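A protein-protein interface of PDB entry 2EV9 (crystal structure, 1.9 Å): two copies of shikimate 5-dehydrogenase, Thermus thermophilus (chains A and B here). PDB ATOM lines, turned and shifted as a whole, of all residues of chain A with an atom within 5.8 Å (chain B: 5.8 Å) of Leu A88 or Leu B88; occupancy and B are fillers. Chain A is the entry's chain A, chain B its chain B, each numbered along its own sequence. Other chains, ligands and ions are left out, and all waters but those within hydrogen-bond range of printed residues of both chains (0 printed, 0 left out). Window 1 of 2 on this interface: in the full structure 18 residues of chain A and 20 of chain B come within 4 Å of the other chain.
Of the printed residues of chain B, Leu A88 touches Leu B88. Of the printed residues of chain B, Phe A97 touches Val B90. Of the printed residues of chain B, Trp A243 touches Arg B55 (3.4 Å). Of the printed residues of chain A, Arg B55 touches Arg A55, Leu A242 and Trp A243. Val B57 touches none of the printed residues of chain A. Printed residues of chain A within 4 Å of Leu B88: Leu A88. Of the printed residues of chain A, Phe B95 touches Phe A95. The nearest printed residue of chain B that does not touch Leu A88 is Val B90 (4.5 Å). The nearest printed residue of chain A that does not touch Leu B88 is Val A90 (4.5 Å).
Among the printed residues, merely in contact across the chains: Phe A95 with Phe B95 (3.2 Å), Phe A97 with Val B90 (3.5 Å), Val A90 with Phe B97 (3.5 Å), Arg A55 with Arg B55 (3.7 Å), Val A90 with Leu B242 (3.8 Å), Phe A95 with Phe B97 (3.9 Å), Leu A242 with Val B90 (3.9 Å) and Leu A88 with Leu B88 (3.99 Å).
Arg B55 touches its own counterpart, Arg A55. Leu B88 touches its own counterpart, Leu A88. Val A90 touches Phe B97, and with the chains exchanged Phe A97 touches Val B90. Phe A95 touches Phe B97, but with the chains exchanged Phe A97 does not touch Phe B95 (4.3 Å). 15 positions are printed for both chains. Of the 12 pairs that touch across the chains among the printed residues, 11 have their exchanged pair printed and touching as well.
The indole nitrogen (NE1) of Trp A243 lies within hydrogen-bond range of the backbone carbonyl oxygen (O) of Val A87, at 2.8 Å. The backbone NH (N) of Leu A88 lies within hydrogen-bond range of the backbone carbonyl oxygen (O) of Phe A95 (3.0 Å). N of Gln B89 is in hydrogen-bond range of O of Arg B55, at 2.8 Å. NE of Arg B55 is in hydrogen-bond range of O of Trp B243 (2.8 Å). O of Thr B86 is in hydrogen-bond range of N of Phe B97 (2.7 Å). The backbone carbonyl oxygen (O) of Val B87 is in hydrogen-bond range of the indole nitrogen (NE1) of Trp B243, at 2.9 Å.
Of the 15 printed residues of chain A, 7 touch a printed residue of chain B. Printed residues of chain A that touch a printed residue of chain B: Arg A55, Leu A88, Val A90, Phe A95, Phe A97, Leu A242 and Trp A243. Hydrophobic or aromatic side chains of chain A that line the printed part of chain B: Leu A88, Val A90, Phe A95 and Phe A97. Among the printed residues, 12 pairs touch across the chains.
The guanidinium group (NH2) of Arg A55 lies within hydrogen-bond range of the backbone carbonyl oxygen (O) of Leu B242, 2.9 Å away. NH2 of Arg A55 sits at hydrogen-bond distance from O of Trp B243 (3.4 Å). NH2 of Arg B55 lies within hydrogen-bond range of O of Leu A242, at 2.9 Å. The guanidinium group (NH2) of Arg B55 is in hydrogen-bond range of the backbone carbonyl oxygen (O) of Trp A243 (3.4 Å).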
ATOM      1  N   ARG A  55      -7.626 -31.582 -15.452  1.00  0.00           N
ATOM      2  CA  ARG A  55      -7.828 -30.501 -16.403  1.00  0.00           C
ATOM      3  C   ARG A  55      -8.519 -29.340 -15.683  1.00  0.00           C
ATOM      4  O   ARG A  55      -8.268 -28.168 -15.975  1.00  0.00           O
ATOM      5  CB  ARG A  55      -8.705 -30.979 -17.561  1.00  0.00           C
ATOM      6  CG  ARG A  55      -9.214 -29.860 -18.455  1.00  0.00           C
ATOM      7  CD  ARG A  55      -8.093 -29.172 -19.216  1.00  0.00           C
ATOM      8  NE  ARG A  55      -8.620 -28.157 -20.128  1.00  0.00           N
ATOM      9  CZ  ARG A  55      -7.874 -27.433 -20.956  1.00  0.00           C
ATOM     10  NH1 ARG A  55      -6.562 -27.608 -20.994  1.00  0.00           N
ATOM     11  NH2 ARG A  55      -8.441 -26.530 -21.744  1.00  0.00           N
ATOM     12  N   GLY A  56      -9.394 -29.678 -14.741  1.00  0.00           N
ATOM     13  CA  GLY A  56     -10.099 -28.653 -13.996  1.00  0.00           C
ATOM     14  C   GLY A  56     -10.907 -29.213 -12.843  1.00  0.00           C
ATOM     15  O   GLY A  56     -11.206 -30.410 -12.793  1.00  0.00           O
ATOM     16  N   VAL A  57     -11.253 -28.348 -11.899  1.00  0.00           N
ATOM     17  CA  VAL A  57     -12.051 -28.764 -10.752  1.00  0.00           C
ATOM     18  C   VAL A  57     -12.985 -27.658 -10.279  1.00  0.00           C
ATOM     19  O   VAL A  57     -12.756 -26.478 -10.526  1.00  0.00           O
ATOM     20  CB  VAL A  57     -11.162 -29.171  -9.535  1.00  0.00           C
ATOM     21  CG1 VAL A  57     -10.250 -30.339  -9.903  1.00  0.00           C
ATOM     22  CG2 VAL A  57     -10.346 -27.970  -9.041  1.00  0.00           C
ATOM     23  N   THR A  86     -14.475 -22.505  -9.752  1.00  0.00           N
ATOM     24  CA  THR A  86     -14.017 -23.221 -10.932  1.00  0.00           C
ATOM     25  C   THR A  86     -12.542 -22.975 -11.212  1.00  0.00           C
ATOM     26  O   THR A  86     -12.104 -21.835 -11.353  1.00  0.00           O
ATOM     27  CB  THR A  86     -14.826 -22.807 -12.182  1.00  0.00           C
ATOM     28  OG1 THR A  86     -16.195 -23.190 -12.013  1.00  0.00           O
ATOM     29  CG2 THR A  86     -14.263 -23.479 -13.436  1.00  0.00           C
ATOM     30  N   VAL A  87     -11.783 -24.059 -11.304  1.00  0.00           N
ATOM     31  CA  VAL A  87     -10.359 -23.959 -11.575  1.00  0.00           C
ATOM     32  C   VAL A  87     -10.005 -24.678 -12.867  1.00  0.00           C
ATOM     33  O   VAL A  87     -10.485 -25.778 -13.114  1.00  0.00           O
ATOM     34  CB  VAL A  87      -9.532 -24.585 -10.439  1.00  0.00           C
ATOM     35  CG1 VAL A  87      -8.052 -24.531 -10.787  1.00  0.00           C
ATOM     36  CG2 VAL A  87      -9.808 -23.858  -9.134  1.00  0.00           C
ATOM     37  N   LEU A  88      -9.174 -24.038 -13.686  1.00  0.00           N
ATOM     38  CA  LEU A  88      -8.712 -24.606 -14.953  1.00  0.00           C
ATOM     39  C   LEU A  88      -7.203 -24.860 -14.869  1.00  0.00           C
ATOM     40  O   LEU A  88      -6.450 -23.975 -14.455  1.00  0.00           O
ATOM     41  CB  LEU A  88      -8.981 -23.638 -16.108  1.00  0.00           C
ATOM     42  CG  LEU A  88      -8.166 -23.928 -17.375  1.00  0.00           C
ATOM     43  CD1 LEU A  88      -8.624 -25.253 -17.978  1.00  0.00           C
ATOM     44  CD2 LEU A  88      -8.322 -22.788 -18.372  1.00  0.00           C
ATOM     45  N   GLN A  89      -6.767 -26.053 -15.272  1.00  0.00           N
ATOM     46  CA  GLN A  89      -5.341 -26.408 -15.243  1.00  0.00           C
ATOM     47  C   GLN A  89      -4.745 -26.512 -16.653  1.00  0.00           C
ATOM     48  O   GLN A  89      -5.251 -27.249 -17.499  1.00  0.00           O
ATOM     49  CB  GLN A  89      -5.148 -27.742 -14.503  1.00  0.00           C
ATOM     50  CG  GLN A  89      -3.689 -28.244 -14.365  1.00  0.00           C
ATOM     51  CD  GLN A  89      -3.153 -28.915 -15.628  1.00  0.00           C
ATOM     52  OE1 GLN A  89      -2.303 -28.362 -16.330  1.00  0.00           O
ATOM     53  NE2 GLN A  89      -3.654 -30.108 -15.923  1.00  0.00           N
ATOM     54  N   VAL A  90      -3.687 -25.744 -16.899  1.00  0.00           N
ATOM     55  CA  VAL A  90      -2.981 -25.755 -18.179  1.00  0.00           C
ATOM     56  C   VAL A  90      -1.494 -25.570 -17.894  1.00  0.00           C
ATOM     57  O   VAL A  90      -1.100 -24.632 -17.196  1.00  0.00           O
ATOM     58  CB  VAL A  90      -3.454 -24.633 -19.133  1.00  0.00           C
ATOM     59  CG1 VAL A  90      -4.852 -24.952 -19.661  1.00  0.00           C
ATOM     60  CG2 VAL A  90      -3.462 -23.297 -18.413  1.00  0.00           C
ATOM     61  N   ARG A  93      -0.324 -24.769 -14.550  1.00  0.00           N
ATOM     62  CA  ARG A  93      -0.728 -23.491 -13.971  1.00  0.00           C
ATOM     63  C   ARG A  93      -2.216 -23.556 -13.611  1.00  0.00           C
ATOM     64  O   ARG A  93      -2.981 -24.289 -14.238  1.00  0.00           O
ATOM     65  CB  ARG A  93      -0.482 -22.350 -14.963  1.00  0.00           C
ATOM     66  CG  ARG A  93       0.887 -22.365 -15.630  1.00  0.00           C
ATOM     67  CD  ARG A  93       2.032 -22.283 -14.627  1.00  0.00           C
ATOM     68  NE  ARG A  93       3.333 -22.337 -15.298  1.00  0.00           N
ATOM     69  CZ  ARG A  93       4.507 -22.222 -14.680  1.00  0.00           C
ATOM     70  NH1 ARG A  93       4.558 -22.046 -13.365  1.00  0.00           N
ATOM     71  NH2 ARG A  93       5.634 -22.282 -15.376  1.00  0.00           N
ATOM     72  N   LEU A  94      -2.620 -22.799 -12.595  1.00  0.00           N
ATOM     73  CA  LEU A  94      -4.015 -22.790 -12.161  1.00  0.00           C
ATOM     74  C   LEU A  94      -4.661 -21.415 -12.279  1.00  0.00           C
ATOM     75  O   LEU A  94      -4.136 -20.417 -11.778  1.00  0.00           O
ATOM     76  CB  LEU A  94      -4.129 -23.281 -10.718  1.00  0.00           C
ATOM     77  CG  LEU A  94      -3.606 -24.690 -10.435  1.00  0.00           C
ATOM     78  CD1 LEU A  94      -3.788 -25.004  -8.957  1.00  0.00           C
ATOM     79  CD2 LEU A  94      -4.341 -25.708 -11.296  1.00  0.00           C
ATOM     80  N   PHE A  95      -5.804 -21.377 -12.954  1.00  0.00           N
ATOM     81  CA  PHE A  95      -6.545 -20.142 -13.160  1.00  0.00           C
ATOM     82  C   PHE A  95      -7.877 -20.283 -12.441  1.00  0.00           C
ATOM     83  O   PHE A  95      -8.553 -21.307 -12.580  1.00  0.00           O
ATOM     84  CB  PHE A  95      -6.786 -19.923 -14.655  1.00  0.00           C
ATOM     85  CG  PHE A  95      -5.528 -19.872 -15.475  1.00  0.00           C
ATOM     86  CD1 PHE A  95      -5.577 -20.077 -16.851  1.00  0.00           C
ATOM     87  CD2 PHE A  95      -4.295 -19.620 -14.878  1.00  0.00           C
ATOM     88  CE1 PHE A  95      -4.411 -20.033 -17.619  1.00  0.00           C
ATOM     89  CE2 PHE A  95      -3.127 -19.574 -15.638  1.00  0.00           C
ATOM     90  CZ  PHE A  95      -3.185 -19.781 -17.008  1.00  0.00           C
ATOM     91  N   GLY A  96      -8.247 -19.260 -11.674  1.00  0.00           N
ATOM     92  CA  GLY A  96      -9.495 -19.306 -10.936  1.00  0.00           C
ATOM     93  C   GLY A  96     -10.583 -18.427 -11.522  1.00  0.00           C
ATOM     94  O   GLY A  96     -10.334 -17.282 -11.907  1.00  0.00           O
ATOM     95  N   PHE A  97     -11.795 -18.970 -11.588  1.00  0.00           N
ATOM     96  CA  PHE A  97     -12.944 -18.243 -12.119  1.00  0.00           C
ATOM     97  C   PHE A  97     -14.152 -18.461 -11.211  1.00  0.00           C
ATOM     98  O   PHE A  97     -14.121 -19.281 -10.292  1.00  0.00           O
ATOM     99  CB  PHE A  97     -13.320 -18.743 -13.520  1.00  0.00           C
ATOM    100  CG  PHE A  97     -12.185 -18.726 -14.503  1.00  0.00           C
ATOM    101  CD1 PHE A  97     -11.241 -19.753 -14.517  1.00  0.00           C
ATOM    102  CD2 PHE A  97     -12.069 -17.694 -15.432  1.00  0.00           C
ATOM    103  CE1 PHE A  97     -10.203 -19.752 -15.447  1.00  0.00           C
ATOM    104  CE2 PHE A  97     -11.035 -17.682 -16.367  1.00  0.00           C
ATOM    105  CZ  PHE A  97     -10.100 -18.715 -16.376  1.00  0.00           C
ATOM    106  N   LEU A 242     -15.577 -23.511 -19.670  1.00  0.00           N
ATOM    107  CA  LEU A 242     -14.298 -22.905 -19.318  1.00  0.00           C
ATOM    108  C   LEU A 242     -13.188 -23.932 -19.546  1.00  0.00           C
ATOM    109  O   LEU A 242     -12.101 -23.598 -20.025  1.00  0.00           O
ATOM    110  CB  LEU A 242     -14.274 -22.475 -17.845  1.00  0.00           C
ATOM    111  CG  LEU A 242     -14.964 -21.183 -17.410  1.00  0.00           C
ATOM    112  CD1 LEU A 242     -14.695 -20.940 -15.931  1.00  0.00           C
ATOM    113  CD2 LEU A 242     -14.445 -20.018 -18.236  1.00  0.00           C
ATOM    114  N   TRP A 243     -13.474 -25.184 -19.198  1.00  0.00           N
ATOM    115  CA  TRP A 243     -12.503 -26.258 -19.332  1.00  0.00           C
ATOM    116  C   TRP A 243     -12.278 -26.791 -20.744  1.00  0.00           C
ATOM    117  O   TRP A 243     -11.150 -27.106 -21.112  1.00  0.00           O
ATOM    118  CB  TRP A 243     -12.897 -27.453 -18.442  1.00  0.00           C
ATOM    119  CG  TRP A 243     -12.972 -27.165 -16.973  1.00  0.00           C
ATOM    120  CD1 TRP A 243     -12.173 -26.317 -16.259  1.00  0.00           C
ATOM    121  CD2 TRP A 243     -13.881 -27.745 -16.033  1.00  0.00           C
ATOM    122  NE1 TRP A 243     -12.531 -26.332 -14.933  1.00  0.00           N
ATOM    123  CE2 TRP A 243     -13.576 -27.200 -14.767  1.00  0.00           C
ATOM    124  CE3 TRP A 243     -14.923 -28.673 -16.136  1.00  0.00           C
ATOM    125  CZ2 TRP A 243     -14.279 -27.550 -13.612  1.00  0.00           C
ATOM    126  CZ3 TRP A 243     -15.623 -29.021 -14.985  1.00  0.00           C
ATOM    127  CH2 TRP A 243     -15.296 -28.458 -13.740  1.00  0.00           C
ATOM    128  N   ARG B  55     -11.707 -19.547 -29.366  1.00  0.00           N
ATOM    129  CA  ARG B  55     -11.372 -20.274 -28.151  1.00  0.00           C
ATOM    130  C   ARG B  55      -9.854 -20.180 -27.987  1.00  0.00           C
ATOM    131  O   ARG B  55      -9.330 -20.085 -26.871  1.00  0.00           O
ATOM    132  CB  ARG B  55     -11.792 -21.745 -28.280  1.00  0.00           C
ATOM    133  CG  ARG B  55     -11.236 -22.653 -27.190  1.00  0.00           C
ATOM    134  CD  ARG B  55     -11.799 -22.325 -25.805  1.00  0.00           C
ATOM    135  NE  ARG B  55     -11.258 -23.232 -24.790  1.00  0.00           N
ATOM    136  CZ  ARG B  55     -11.633 -23.257 -23.513  1.00  0.00           C
ATOM    137  NH1 ARG B  55     -12.564 -22.419 -23.072  1.00  0.00           N
ATOM    138  NH2 ARG B  55     -11.077 -24.129 -22.677  1.00  0.00           N
ATOM    139  N   GLY B  56      -9.152 -20.206 -29.116  1.00  0.00           N
ATOM    140  CA  GLY B  56      -7.703 -20.120 -29.081  1.00  0.00           C
ATOM    141  C   GLY B  56      -7.083 -19.871 -30.441  1.00  0.00           C
ATOM    142  O   GLY B  56      -7.743 -19.994 -31.479  1.00  0.00           O
ATOM    143  N   VAL B  57      -5.809 -19.502 -30.436  1.00  0.00           N
ATOM    144  CA  VAL B  57      -5.087 -19.246 -31.675  1.00  0.00           C
ATOM    145  C   VAL B  57      -3.596 -19.446 -31.488  1.00  0.00           C
ATOM    146  O   VAL B  57      -3.071 -19.362 -30.373  1.00  0.00           O
ATOM    147  CB  VAL B  57      -5.293 -17.785 -32.218  1.00  0.00           C
ATOM    148  CG1 VAL B  57      -6.758 -17.528 -32.544  1.00  0.00           C
ATOM    149  CG2 VAL B  57      -4.780 -16.769 -31.211  1.00  0.00           C
ATOM    150  N   THR B  86       0.974 -19.645 -28.538  1.00  0.00           N
ATOM    151  CA  THR B  86      -0.350 -20.177 -28.247  1.00  0.00           C
ATOM    152  C   THR B  86      -1.164 -19.289 -27.315  1.00  0.00           C
ATOM    153  O   THR B  86      -0.754 -19.004 -26.189  1.00  0.00           O
ATOM    154  CB  THR B  86      -0.244 -21.575 -27.623  1.00  0.00           C
ATOM    155  OG1 THR B  86       0.441 -22.446 -28.532  1.00  0.00           O
ATOM    156  CG2 THR B  86      -1.632 -22.143 -27.320  1.00  0.00           C
ATOM    157  N   VAL B  87      -2.332 -18.868 -27.791  1.00  0.00           N
ATOM    158  CA  VAL B  87      -3.211 -18.019 -27.002  1.00  0.00           C
ATOM    159  C   VAL B  87      -4.523 -18.732 -26.692  1.00  0.00           C
ATOM    160  O   VAL B  87      -5.142 -19.327 -27.571  1.00  0.00           O
ATOM    161  CB  VAL B  87      -3.525 -16.696 -27.747  1.00  0.00           C
ATOM    162  CG1 VAL B  87      -4.435 -15.817 -26.896  1.00  0.00           C
ATOM    163  CG2 VAL B  87      -2.229 -15.954 -28.067  1.00  0.00           C
ATOM    164  N   LEU B  88      -4.933 -18.672 -25.431  1.00  0.00           N
ATOM    165  CA  LEU B  88      -6.188 -19.272 -24.988  1.00  0.00           C
ATOM    166  C   LEU B  88      -7.142 -18.162 -24.552  1.00  0.00           C
ATOM    167  O   LEU B  88      -6.738 -17.234 -23.843  1.00  0.00           O
ATOM    168  CB  LEU B  88      -5.953 -20.216 -23.804  1.00  0.00           C
ATOM    169  CG  LEU B  88      -7.176 -20.596 -22.956  1.00  0.00           C
ATOM    170  CD1 LEU B  88      -8.177 -21.376 -23.791  1.00  0.00           C
ATOM    171  CD2 LEU B  88      -6.716 -21.421 -21.762  1.00  0.00           C
ATOM    172  N   GLN B  89      -8.400 -18.260 -24.976  1.00  0.00           N
ATOM    173  CA  GLN B  89      -9.421 -17.276 -24.606  1.00  0.00           C
ATOM    174  C   GLN B  89     -10.521 -17.919 -23.765  1.00  0.00           C
ATOM    175  O   GLN B  89     -11.171 -18.870 -24.198  1.00  0.00           O
ATOM    176  CB  GLN B  89     -10.051 -16.649 -25.853  1.00  0.00           C
ATOM    177  CG  GLN B  89     -11.138 -15.591 -25.564  1.00  0.00           C
ATOM    178  CD  GLN B  89     -12.500 -16.188 -25.228  1.00  0.00           C
ATOM    179  OE1 GLN B  89     -12.941 -16.165 -24.076  1.00  0.00           O
ATOM    180  NE2 GLN B  89     -13.172 -16.729 -26.239  1.00  0.00           N
ATOM    181  N   VAL B  90     -10.705 -17.397 -22.556  1.00  0.00           N
ATOM    182  CA  VAL B  90     -11.727 -17.862 -21.633  1.00  0.00           C
ATOM    183  C   VAL B  90     -12.313 -16.624 -20.965  1.00  0.00           C
ATOM    184  O   VAL B  90     -11.572 -15.770 -20.479  1.00  0.00           O
ATOM    185  CB  VAL B  90     -11.143 -18.797 -20.551  1.00  0.00           C
ATOM    186  CG1 VAL B  90     -10.682 -20.103 -21.183  1.00  0.00           C
ATOM    187  CG2 VAL B  90      -9.983 -18.134 -19.844  1.00  0.00           C
ATOM    188  N   ARG B  93     -10.901 -13.256 -21.599  1.00  0.00           N
ATOM    189  CA  ARG B  93      -9.516 -13.012 -21.196  1.00  0.00           C
ATOM    190  C   ARG B  93      -8.565 -13.821 -22.080  1.00  0.00           C
ATOM    191  O   ARG B  93      -8.911 -14.908 -22.549  1.00  0.00           O
ATOM    192  CB  ARG B  93      -9.304 -13.405 -19.731  1.00  0.00           C
ATOM    193  CG  ARG B  93     -10.399 -12.926 -18.781  1.00  0.00           C
ATOM    194  CD  ARG B  93     -10.556 -11.405 -18.753  1.00  0.00           C
ATOM    195  NE  ARG B  93     -11.640 -11.010 -17.854  1.00  0.00           N
ATOM    196  CZ  ARG B  93     -12.027  -9.757 -17.637  1.00  0.00           C
ATOM    197  NH1 ARG B  93     -11.423  -8.750 -18.255  1.00  0.00           N
ATOM    198  NH2 ARG B  93     -13.026  -9.510 -16.798  1.00  0.00           N
ATOM    199  N   LEU B  94      -7.367 -13.289 -22.302  1.00  0.00           N
ATOM    200  CA  LEU B  94      -6.374 -13.964 -23.130  1.00  0.00           C
ATOM    201  C   LEU B  94      -5.159 -14.371 -22.306  1.00  0.00           C
ATOM    202  O   LEU B  94      -4.630 -13.581 -21.523  1.00  0.00           O
ATOM    203  CB  LEU B  94      -5.929 -13.057 -24.285  1.00  0.00           C
ATOM    204  CG  LEU B  94      -7.011 -12.547 -25.242  1.00  0.00           C
ATOM    205  CD1 LEU B  94      -6.356 -11.736 -26.364  1.00  0.00           C
ATOM    206  CD2 LEU B  94      -7.800 -13.713 -25.819  1.00  0.00           C
ATOM    207  N   PHE B  95      -4.732 -15.618 -22.485  1.00  0.00           N
ATOM    208  CA  PHE B  95      -3.572 -16.160 -21.784  1.00  0.00           C
ATOM    209  C   PHE B  95      -2.561 -16.627 -22.831  1.00  0.00           C
ATOM    210  O   PHE B  95      -2.928 -17.273 -23.814  1.00  0.00           O
ATOM    211  CB  PHE B  95      -3.982 -17.339 -20.899  1.00  0.00           C
ATOM    212  CG  PHE B  95      -5.025 -16.993 -19.872  1.00  0.00           C
ATOM    213  CD1 PHE B  95      -6.329 -16.704 -20.256  1.00  0.00           C
ATOM    214  CD2 PHE B  95      -4.696 -16.938 -18.524  1.00  0.00           C
ATOM    215  CE1 PHE B  95      -7.295 -16.361 -19.306  1.00  0.00           C
ATOM    216  CE2 PHE B  95      -5.652 -16.599 -17.568  1.00  0.00           C
ATOM    217  CZ  PHE B  95      -6.955 -16.309 -17.962  1.00  0.00           C
ATOM    218  N   GLY B  96      -1.291 -16.301 -22.623  1.00  0.00           N
ATOM    219  CA  GLY B  96      -0.272 -16.688 -23.584  1.00  0.00           C
ATOM    220  C   GLY B  96       0.662 -17.794 -23.140  1.00  0.00           C
ATOM    221  O   GLY B  96       1.137 -17.811 -21.997  1.00  0.00           O
ATOM    222  N   PHE B  97       0.929 -18.726 -24.053  1.00  0.00           N
ATOM    223  CA  PHE B  97       1.819 -19.845 -23.776  1.00  0.00           C
ATOM    224  C   PHE B  97       2.790 -20.061 -24.930  1.00  0.00           C
ATOM    225  O   PHE B  97       2.657 -19.461 -25.997  1.00  0.00           O
ATOM    226  CB  PHE B  97       1.028 -21.140 -23.577  1.00  0.00           C
ATOM    227  CG  PHE B  97      -0.031 -21.050 -22.523  1.00  0.00           C
ATOM    228  CD1 PHE B  97      -1.249 -20.438 -22.793  1.00  0.00           C
ATOM    229  CD2 PHE B  97       0.191 -21.579 -21.256  1.00  0.00           C
ATOM    230  CE1 PHE B  97      -2.235 -20.356 -21.812  1.00  0.00           C
ATOM    231  CE2 PHE B  97      -0.787 -21.501 -20.270  1.00  0.00           C
ATOM    232  CZ  PHE B  97      -2.002 -20.887 -20.552  1.00  0.00           C
ATOM    233  N   LEU B 242      -4.159 -27.672 -24.782  1.00  0.00           N
ATOM    234  CA  LEU B 242      -4.254 -26.468 -23.969  1.00  0.00           C
ATOM    235  C   LEU B 242      -5.626 -25.800 -24.158  1.00  0.00           C
ATOM    236  O   LEU B 242      -6.235 -25.305 -23.205  1.00  0.00           O
ATOM    237  CB  LEU B 242      -3.121 -25.524 -24.369  1.00  0.00           C
ATOM    238  CG  LEU B 242      -2.770 -24.349 -23.469  1.00  0.00           C
ATOM    239  CD1 LEU B 242      -1.270 -24.100 -23.534  1.00  0.00           C
ATOM    240  CD2 LEU B 242      -3.562 -23.120 -23.903  1.00  0.00           C
ATOM    241  N   TRP B 243      -6.130 -25.811 -25.386  1.00  0.00           N
ATOM    242  CA  TRP B 243      -7.425 -25.201 -25.660  1.00  0.00           C
ATOM    243  C   TRP B 243      -8.614 -26.049 -25.236  1.00  0.00           C
ATOM    244  O   TRP B 243      -9.620 -25.521 -24.784  1.00  0.00           O
ATOM    245  CB  TRP B 243      -7.579 -24.900 -27.154  1.00  0.00           C
ATOM    246  CG  TRP B 243      -6.573 -23.949 -27.710  1.00  0.00           C
ATOM    247  CD1 TRP B 243      -6.089 -22.823 -27.111  1.00  0.00           C
ATOM    248  CD2 TRP B 243      -5.957 -24.015 -28.999  1.00  0.00           C
ATOM    249  NE1 TRP B 243      -5.209 -22.183 -27.948  1.00  0.00           N
ATOM    250  CE2 TRP B 243      -5.110 -22.895 -29.115  1.00  0.00           C
ATOM    251  CE3 TRP B 243      -6.043 -24.914 -30.074  1.00  0.00           C
ATOM    252  CZ2 TRP B 243      -4.350 -22.646 -30.263  1.00  0.00           C
ATOM    253  CZ3 TRP B 243      -5.291 -24.669 -31.212  1.00  0.00           C
ATOM    254  CH2 TRP B 243      -4.453 -23.541 -31.298  1.00  0.00           C
